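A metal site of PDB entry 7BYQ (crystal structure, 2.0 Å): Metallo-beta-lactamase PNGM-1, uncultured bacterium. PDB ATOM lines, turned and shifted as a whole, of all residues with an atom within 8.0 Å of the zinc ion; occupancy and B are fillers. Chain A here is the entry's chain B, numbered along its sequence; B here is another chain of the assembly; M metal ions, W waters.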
ATOM      1  N   MET A  39      28.409  18.552   5.496  1.00  0.00           N
ATOM      2  CA  MET A  39      27.766  17.442   4.740  1.00  0.00           C
ATOM      3  C   MET A  39      26.615  16.791   5.511  1.00  0.00           C
ATOM      4  O   MET A  39      26.080  17.394   6.435  1.00  0.00           O
ATOM      5  CB  MET A  39      28.871  16.440   4.393  1.00  0.00           C
ATOM      6  CG  MET A  39      29.730  16.029   5.595  1.00  0.00           C
ATOM      7  SD  MET A  39      31.482  16.020   5.151  1.00  0.00           S
ATOM      8  CE  MET A  39      31.914  14.385   5.757  1.00  0.00           C
ATOM      9  N   PRO A  40      26.157  15.547   5.188  1.00  0.00           N
ATOM     10  CA  PRO A  40      24.844  15.082   5.639  1.00  0.00           C
ATOM     11  C   PRO A  40      24.720  14.926   7.160  1.00  0.00           C
ATOM     12  O   PRO A  40      23.629  15.158   7.677  1.00  0.00           O
ATOM     13  CB  PRO A  40      24.684  13.716   4.956  1.00  0.00           C
ATOM     14  CG  PRO A  40      26.106  13.214   4.796  1.00  0.00           C
ATOM     15  CD  PRO A  40      26.912  14.464   4.509  1.00  0.00           C
ATOM     16  N   ALA A  49      24.261  22.666   4.285  1.00  0.00           N
ATOM     17  CA  ALA A  49      24.454  23.734   3.268  1.00  0.00           C
ATOM     18  C   ALA A  49      23.344  24.779   3.404  1.00  0.00           C
ATOM     19  O   ALA A  49      22.179  24.425   3.183  1.00  0.00           O
ATOM     20  CB  ALA A  49      24.470  23.138   1.882  1.00  0.00           C
ATOM     21  N   ASP A  64      20.089  27.354  -0.702  1.00  0.00           N
ATOM     22  CA  ASP A  64      20.093  26.112   0.122  1.00  0.00           C
ATOM     23  C   ASP A  64      19.693  26.470   1.573  1.00  0.00           C
ATOM     24  O   ASP A  64      19.999  27.594   2.045  1.00  0.00           O
ATOM     25  CB  ASP A  64      21.430  25.351  -0.022  1.00  0.00           C
ATOM     26  CG  ASP A  64      21.629  24.729  -1.408  1.00  0.00           C
ATOM     27  OD1 ASP A  64      20.605  24.497  -2.114  1.00  0.00           O
ATOM     28  OD2 ASP A  64      22.795  24.459  -1.772  1.00  0.00           O
ATOM     29  N   THR A  89      19.737  24.312  -4.747  1.00  0.00           N
ATOM     30  CA  THR A  89      20.713  23.658  -5.660  1.00  0.00           C
ATOM     31  C   THR A  89      20.399  22.160  -5.783  1.00  0.00           C
ATOM     32  O   THR A  89      21.027  21.536  -6.641  1.00  0.00           O
ATOM     33  CB  THR A  89      22.163  23.851  -5.179  1.00  0.00           C
ATOM     34  OG1 THR A  89      22.397  23.036  -4.026  1.00  0.00           O
ATOM     35  CG2 THR A  89      22.506  25.281  -4.861  1.00  0.00           C
ATOM     36  N   HIS A  90      19.536  21.617  -4.923  1.00  0.00           N
ATOM     37  CA  HIS A  90      18.912  20.262  -5.055  1.00  0.00           C
ATOM     38  C   HIS A  90      18.158  19.874  -3.785  1.00  0.00           C
ATOM     39  O   HIS A  90      17.898  20.744  -2.949  1.00  0.00           O
ATOM     40  CB  HIS A  90      19.951  19.204  -5.471  1.00  0.00           C
ATOM     41  CG  HIS A  90      21.055  18.973  -4.501  1.00  0.00           C
ATOM     42  ND1 HIS A  90      21.955  19.957  -4.166  1.00  0.00           N
ATOM     43  CD2 HIS A  90      21.420  17.857  -3.831  1.00  0.00           C
ATOM     44  CE1 HIS A  90      22.832  19.465  -3.315  1.00  0.00           C
ATOM     45  NE2 HIS A  90      22.529  18.172  -3.085  1.00  0.00           N
ATOM     46  N   LEU A  91      17.738  18.611  -3.694  1.00  0.00           N
ATOM     47  CA  LEU A  91      16.695  18.139  -2.760  1.00  0.00           C
ATOM     48  C   LEU A  91      17.233  16.967  -1.929  1.00  0.00           C
ATOM     49  O   LEU A  91      16.435  16.119  -1.535  1.00  0.00           O
ATOM     50  CB  LEU A  91      15.461  17.742  -3.578  1.00  0.00           C
ATOM     51  CG  LEU A  91      14.928  18.827  -4.516  1.00  0.00           C
ATOM     52  CD1 LEU A  91      13.823  18.254  -5.405  1.00  0.00           C
ATOM     53  CD2 LEU A  91      14.454  20.041  -3.745  1.00  0.00           C
ATOM     54  N   HIS A  92      18.536  16.949  -1.679  1.00  0.00           N
ATOM     55  CA  HIS A  92      19.116  16.292  -0.473  1.00  0.00           C
ATOM     56  C   HIS A  92      18.514  16.981   0.760  1.00  0.00           C
ATOM     57  O   HIS A  92      18.279  18.221   0.699  1.00  0.00           O
ATOM     58  CB  HIS A  92      20.650  16.323  -0.500  1.00  0.00           C
ATOM     59  CG  HIS A  92      21.270  15.106  -1.086  1.00  0.00           C
ATOM     60  ND1 HIS A  92      22.328  15.156  -1.973  1.00  0.00           N
ATOM     61  CD2 HIS A  92      20.976  13.801  -0.904  1.00  0.00           C
ATOM     62  CE1 HIS A  92      22.634  13.923  -2.336  1.00  0.00           C
ATOM     63  NE2 HIS A  92      21.827  13.075  -1.691  1.00  0.00           N
ATOM     64  N   THR A  93      18.247  16.204   1.819  1.00  0.00           N
ATOM     65  CA  THR A  93      17.714  16.732   3.109  1.00  0.00           C
ATOM     66  C   THR A  93      18.718  17.772   3.631  1.00  0.00           C
ATOM     67  O   THR A  93      18.282  18.791   4.197  1.00  0.00           O
ATOM     68  CB  THR A  93      17.328  15.587   4.067  1.00  0.00           C
ATOM     69  OG1 THR A  93      18.432  14.786   4.503  1.00  0.00           O
ATOM     70  CG2 THR A  93      16.329  14.625   3.446  1.00  0.00           C
ATOM     71  N   ASP A  94      20.025  17.564   3.360  1.00  0.00           N
ATOM     72  CA  ASP A  94      21.126  18.469   3.799  1.00  0.00           C
ATOM     73  C   ASP A  94      21.221  19.693   2.878  1.00  0.00           C
ATOM     74  O   ASP A  94      22.233  20.400   2.966  1.00  0.00           O
ATOM     75  CB  ASP A  94      22.451  17.699   3.934  1.00  0.00           C
ATOM     76  CG  ASP A  94      23.237  17.405   2.659  1.00  0.00           C
ATOM     77  OD1 ASP A  94      22.745  16.590   1.821  1.00  0.00           O
ATOM     78  OD2 ASP A  94      24.361  17.940   2.532  1.00  0.00           O
ATOM     79  N   HIS A  95      20.191  19.993   2.076  1.00  0.00           N
ATOM     80  CA  HIS A  95      20.135  21.257   1.281  1.00  0.00           C
ATOM     81  C   HIS A  95      18.813  22.005   1.475  1.00  0.00           C
ATOM     82  O   HIS A  95      18.853  23.230   1.349  1.00  0.00           O
ATOM     83  CB  HIS A  95      20.483  20.975  -0.195  1.00  0.00           C
ATOM     84  CG  HIS A  95      21.937  20.728  -0.383  1.00  0.00           C
ATOM     85  ND1 HIS A  95      22.805  21.710  -0.807  1.00  0.00           N
ATOM     86  CD2 HIS A  95      22.689  19.622  -0.157  1.00  0.00           C
ATOM     87  CE1 HIS A  95      24.022  21.224  -0.867  1.00  0.00           C
ATOM     88  NE2 HIS A  95      23.978  19.952  -0.448  1.00  0.00           N
ATOM     89  N   HIS A 187      25.688  14.547  -9.529  1.00  0.00           N
ATOM     90  CA  HIS A 187      25.577  14.242  -8.079  1.00  0.00           C
ATOM     91  C   HIS A 187      24.293  13.450  -7.779  1.00  0.00           C
ATOM     92  O   HIS A 187      23.192  14.017  -7.949  1.00  0.00           O
ATOM     93  CB  HIS A 187      25.656  15.558  -7.283  1.00  0.00           C
ATOM     94  CG  HIS A 187      25.386  15.423  -5.812  1.00  0.00           C
ATOM     95  ND1 HIS A 187      26.338  14.916  -4.933  1.00  0.00           N
ATOM     96  CD2 HIS A 187      24.325  15.772  -5.061  1.00  0.00           C
ATOM     97  CE1 HIS A 187      25.856  14.929  -3.711  1.00  0.00           C
ATOM     98  NE2 HIS A 187      24.623  15.483  -3.755  1.00  0.00           N
ATOM     99  N   ALA A 188      24.443  12.187  -7.352  1.00  0.00           N
ATOM    100  CA  ALA A 188      23.376  11.286  -6.847  1.00  0.00           C
ATOM    101  C   ALA A 188      22.516  10.804  -8.034  1.00  0.00           C
ATOM    102  O   ALA A 188      22.297   9.603  -8.118  1.00  0.00           O
ATOM    103  CB  ALA A 188      22.554  11.974  -5.775  1.00  0.00           C
ATOM    104  N   PRO A 192      20.388  18.177  -9.670  1.00  0.00           N
ATOM    105  CA  PRO A 192      21.162  19.263  -9.020  1.00  0.00           C
ATOM    106  C   PRO A 192      21.853  20.333  -9.876  1.00  0.00           C
ATOM    107  O   PRO A 192      22.586  19.968 -10.804  1.00  0.00           O
ATOM    108  CB  PRO A 192      22.241  18.475  -8.262  1.00  0.00           C
ATOM    109  CG  PRO A 192      21.583  17.159  -7.917  1.00  0.00           C
ATOM    110  CD  PRO A 192      20.677  16.864  -9.091  1.00  0.00           C
ATOM    111  N   GLY A 208      26.716  24.211  -4.911  1.00  0.00           N
ATOM    112  CA  GLY A 208      25.878  23.097  -4.418  1.00  0.00           C
ATOM    113  C   GLY A 208      26.732  21.853  -4.224  1.00  0.00           C
ATOM    114  O   GLY A 208      27.685  21.925  -3.409  1.00  0.00           O
ATOM    115  N   ASP A 209      26.413  20.769  -4.946  1.00  0.00           N
ATOM    116  CA  ASP A 209      27.200  19.508  -4.980  1.00  0.00           C
ATOM    117  C   ASP A 209      27.354  19.021  -6.421  1.00  0.00           C
ATOM    118  O   ASP A 209      26.362  19.103  -7.180  1.00  0.00           O
ATOM    119  CB  ASP A 209      26.537  18.373  -4.190  1.00  0.00           C
ATOM    120  CG  ASP A 209      26.376  18.680  -2.716  1.00  0.00           C
ATOM    121  OD1 ASP A 209      27.384  19.012  -2.059  1.00  0.00           O
ATOM    122  OD2 ASP A 209      25.231  18.601  -2.249  1.00  0.00           O
ATOM    123  N   THR A 210      28.533  18.495  -6.766  1.00  0.00           N
ATOM    124  CA  THR A 210      28.912  18.144  -8.151  1.00  0.00           C
ATOM    125  C   THR A 210      30.291  17.469  -8.181  1.00  0.00           C
ATOM    126  O   THR A 210      31.276  18.060  -7.693  1.00  0.00           O
ATOM    127  CB  THR A 210      28.881  19.382  -9.066  1.00  0.00           C
ATOM    128  OG1 THR A 210      28.761  18.916 -10.413  1.00  0.00           O
ATOM    129  CG2 THR A 210      30.076  20.297  -8.919  1.00  0.00           C
ATOM    130  N   GLU A 229      31.946  22.788  -3.994  1.00  0.00           N
ATOM    131  CA  GLU A 229      32.197  21.490  -3.322  1.00  0.00           C
ATOM    132  C   GLU A 229      33.708  21.305  -3.162  1.00  0.00           C
ATOM    133  O   GLU A 229      34.455  21.503  -4.168  1.00  0.00           O
ATOM    134  CB  GLU A 229      31.566  20.376  -4.155  1.00  0.00           C
ATOM    135  CG  GLU A 229      31.932  18.984  -3.676  1.00  0.00           C
ATOM    136  CD  GLU A 229      30.943  17.888  -4.035  1.00  0.00           C
ATOM    137  OE1 GLU A 229      29.719  18.118  -3.885  1.00  0.00           O
ATOM    138  OE2 GLU A 229      31.390  16.798  -4.439  1.00  0.00           O
ATOM    139  N   TRP A 231      35.659  18.052  -0.989  1.00  0.00           N
ATOM    140  CA  TRP A 231      35.523  16.826  -0.145  1.00  0.00           C
ATOM    141  C   TRP A 231      36.759  16.656   0.754  1.00  0.00           C
ATOM    142  O   TRP A 231      37.716  17.458   0.628  1.00  0.00           O
ATOM    143  CB  TRP A 231      35.274  15.589  -1.026  1.00  0.00           C
ATOM    144  CG  TRP A 231      34.483  14.520  -0.348  1.00  0.00           C
ATOM    145  CD1 TRP A 231      34.874  13.231  -0.083  1.00  0.00           C
ATOM    146  CD2 TRP A 231      33.142  14.631   0.175  1.00  0.00           C
ATOM    147  NE1 TRP A 231      33.878  12.547   0.550  1.00  0.00           N
ATOM    148  CE2 TRP A 231      32.800  13.368   0.724  1.00  0.00           C
ATOM    149  CE3 TRP A 231      32.199  15.660   0.214  1.00  0.00           C
ATOM    150  CZ2 TRP A 231      31.561  13.132   1.321  1.00  0.00           C
ATOM    151  CZ3 TRP A 231      30.973  15.429   0.810  1.00  0.00           C
ATOM    152  CH2 TRP A 231      30.662  14.183   1.347  1.00  0.00           C
ATOM    153  N   HIS A 256      32.309  12.718  -5.628  1.00  0.00           N
ATOM    154  CA  HIS A 256      32.550  14.087  -5.097  1.00  0.00           C
ATOM    155  C   HIS A 256      33.845  14.686  -5.680  1.00  0.00           C
ATOM    156  O   HIS A 256      34.670  13.905  -6.213  1.00  0.00           O
ATOM    157  CB  HIS A 256      32.522  14.064  -3.562  1.00  0.00           C
ATOM    158  CG  HIS A 256      31.282  13.435  -3.002  1.00  0.00           C
ATOM    159  ND1 HIS A 256      30.088  14.135  -2.869  1.00  0.00           N
ATOM    160  CD2 HIS A 256      31.040  12.196  -2.541  1.00  0.00           C
ATOM    161  CE1 HIS A 256      29.171  13.343  -2.344  1.00  0.00           C
ATOM    162  NE2 HIS A 256      29.734  12.156  -2.126  1.00  0.00           N
ATOM    163  N   TYR A 277      33.749  24.428   0.590  1.00  0.00           N
ATOM    164  CA  TYR A 277      32.744  24.050   1.615  1.00  0.00           C
ATOM    165  C   TYR A 277      32.324  22.600   1.394  1.00  0.00           C
ATOM    166  O   TYR A 277      32.737  22.002   0.376  1.00  0.00           O
ATOM    167  CB  TYR A 277      31.551  25.028   1.572  1.00  0.00           C
ATOM    168  CG  TYR A 277      30.350  24.551   0.804  1.00  0.00           C
ATOM    169  CD1 TYR A 277      30.241  24.703  -0.570  1.00  0.00           C
ATOM    170  CD2 TYR A 277      29.282  23.942   1.466  1.00  0.00           C
ATOM    171  CE1 TYR A 277      29.128  24.264  -1.273  1.00  0.00           C
ATOM    172  CE2 TYR A 277      28.173  23.493   0.785  1.00  0.00           C
ATOM    173  CZ  TYR A 277      28.080  23.664  -0.588  1.00  0.00           C
ATOM    174  OH  TYR A 277      26.961  23.207  -1.234  1.00  0.00           O
ATOM    175  N   TRP B 142      13.410  12.512  -4.185  1.00  0.00           N
ATOM    176  CA  TRP B 142      14.627  12.736  -4.990  1.00  0.00           C
ATOM    177  C   TRP B 142      15.854  12.223  -4.222  1.00  0.00           C
ATOM    178  O   TRP B 142      16.828  11.798  -4.878  1.00  0.00           O
ATOM    179  CB  TRP B 142      14.825  14.204  -5.412  1.00  0.00           C
ATOM    180  CG  TRP B 142      16.102  14.351  -6.182  1.00  0.00           C
ATOM    181  CD1 TRP B 142      16.257  14.245  -7.523  1.00  0.00           C
ATOM    182  CD2 TRP B 142      17.413  14.478  -5.637  1.00  0.00           C
ATOM    183  NE1 TRP B 142      17.575  14.343  -7.870  1.00  0.00           N
ATOM    184  CE2 TRP B 142      18.314  14.496  -6.716  1.00  0.00           C
ATOM    185  CE3 TRP B 142      17.928  14.604  -4.339  1.00  0.00           C
ATOM    186  CZ2 TRP B 142      19.688  14.621  -6.543  1.00  0.00           C
ATOM    187  CZ3 TRP B 142      19.282  14.741  -4.174  1.00  0.00           C
ATOM    188  CH2 TRP B 142      20.153  14.757  -5.257  1.00  0.00           C
ATOM    189  N   ASP B 143      15.813  12.345  -2.889  1.00  0.00           N
ATOM    190  CA  ASP B 143      16.825  11.850  -1.927  1.00  0.00           C
ATOM    191  C   ASP B 143      16.742  10.322  -1.886  1.00  0.00           C
ATOM    192  O   ASP B 143      17.720   9.661  -2.259  1.00  0.00           O
ATOM    193  CB  ASP B 143      16.554  12.501  -0.568  1.00  0.00           C
ATOM    194  CG  ASP B 143      17.607  12.258   0.499  1.00  0.00           C
ATOM    195  OD1 ASP B 143      17.704  11.101   0.973  1.00  0.00           O
ATOM    196  OD2 ASP B 143      18.285  13.236   0.869  1.00  0.00           O
ATOM    197  N   ARG B 147      19.716   7.806  -3.529  1.00  0.00           N
ATOM    198  CA  ARG B 147      20.411   7.016  -2.476  1.00  0.00           C
ATOM    199  C   ARG B 147      20.173   5.519  -2.710  1.00  0.00           C
ATOM    200  O   ARG B 147      21.136   4.732  -2.546  1.00  0.00           O
ATOM    201  CB  ARG B 147      19.937   7.442  -1.089  1.00  0.00           C
ATOM    202  CG  ARG B 147      20.812   6.959   0.066  1.00  0.00           C
ATOM    203  CD  ARG B 147      20.733   7.918   1.236  1.00  0.00           C
ATOM    204  NE  ARG B 147      21.574   9.086   1.015  1.00  0.00           N
ATOM    205  CZ  ARG B 147      21.226  10.354   1.280  1.00  0.00           C
ATOM    206  NH1 ARG B 147      20.040  10.655   1.770  1.00  0.00           N
ATOM    207  NH2 ARG B 147      22.090  11.331   1.036  1.00  0.00           N
HETATM  208 ZN    ZN M   1      23.800  16.671  -1.958  1.00  0.00          ZN
HETATM  209  O   HOH W   1      24.848  16.107   0.298  1.00  0.00           O
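A ring nitrogen (NE2) of His 92 is in hydrogen-bond range of the guanidinium group (NH2) of Arg 147 of chain B (3.2 Å).
The side-chain hydroxyl (OG1) of Thr 89 sits at hydrogen-bond distance from a ring nitrogen (ND1) of His 90 (3.1 Å).
The side-chain carboxylate of Asp 64 lies within hydrogen-bond range of a ring nitrogen (ND1) of His 95.
A ring nitrogen (NE2) of His 95 lies close to the side-chain carboxylate (OD2) of Asp 209.
NE2 of His 95 lies close to NE2 of His 90 (3.5 Å).
O of Asp 94 sits at hydrogen-bond distance from N of Ala 49 (3.3 Å).
Residues that only touch the zinc ion: His 95 and Asp 94.
Six residues have an atom within 4 Å of the zinc ion: His 90, His 92, Asp 94, His 95, His 187 and Asp 209.
The zinc ion is bound by ND1 of His 92, NE2 of His 90, NE2 of His 187, OD2 of Asp 209 and water W1.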
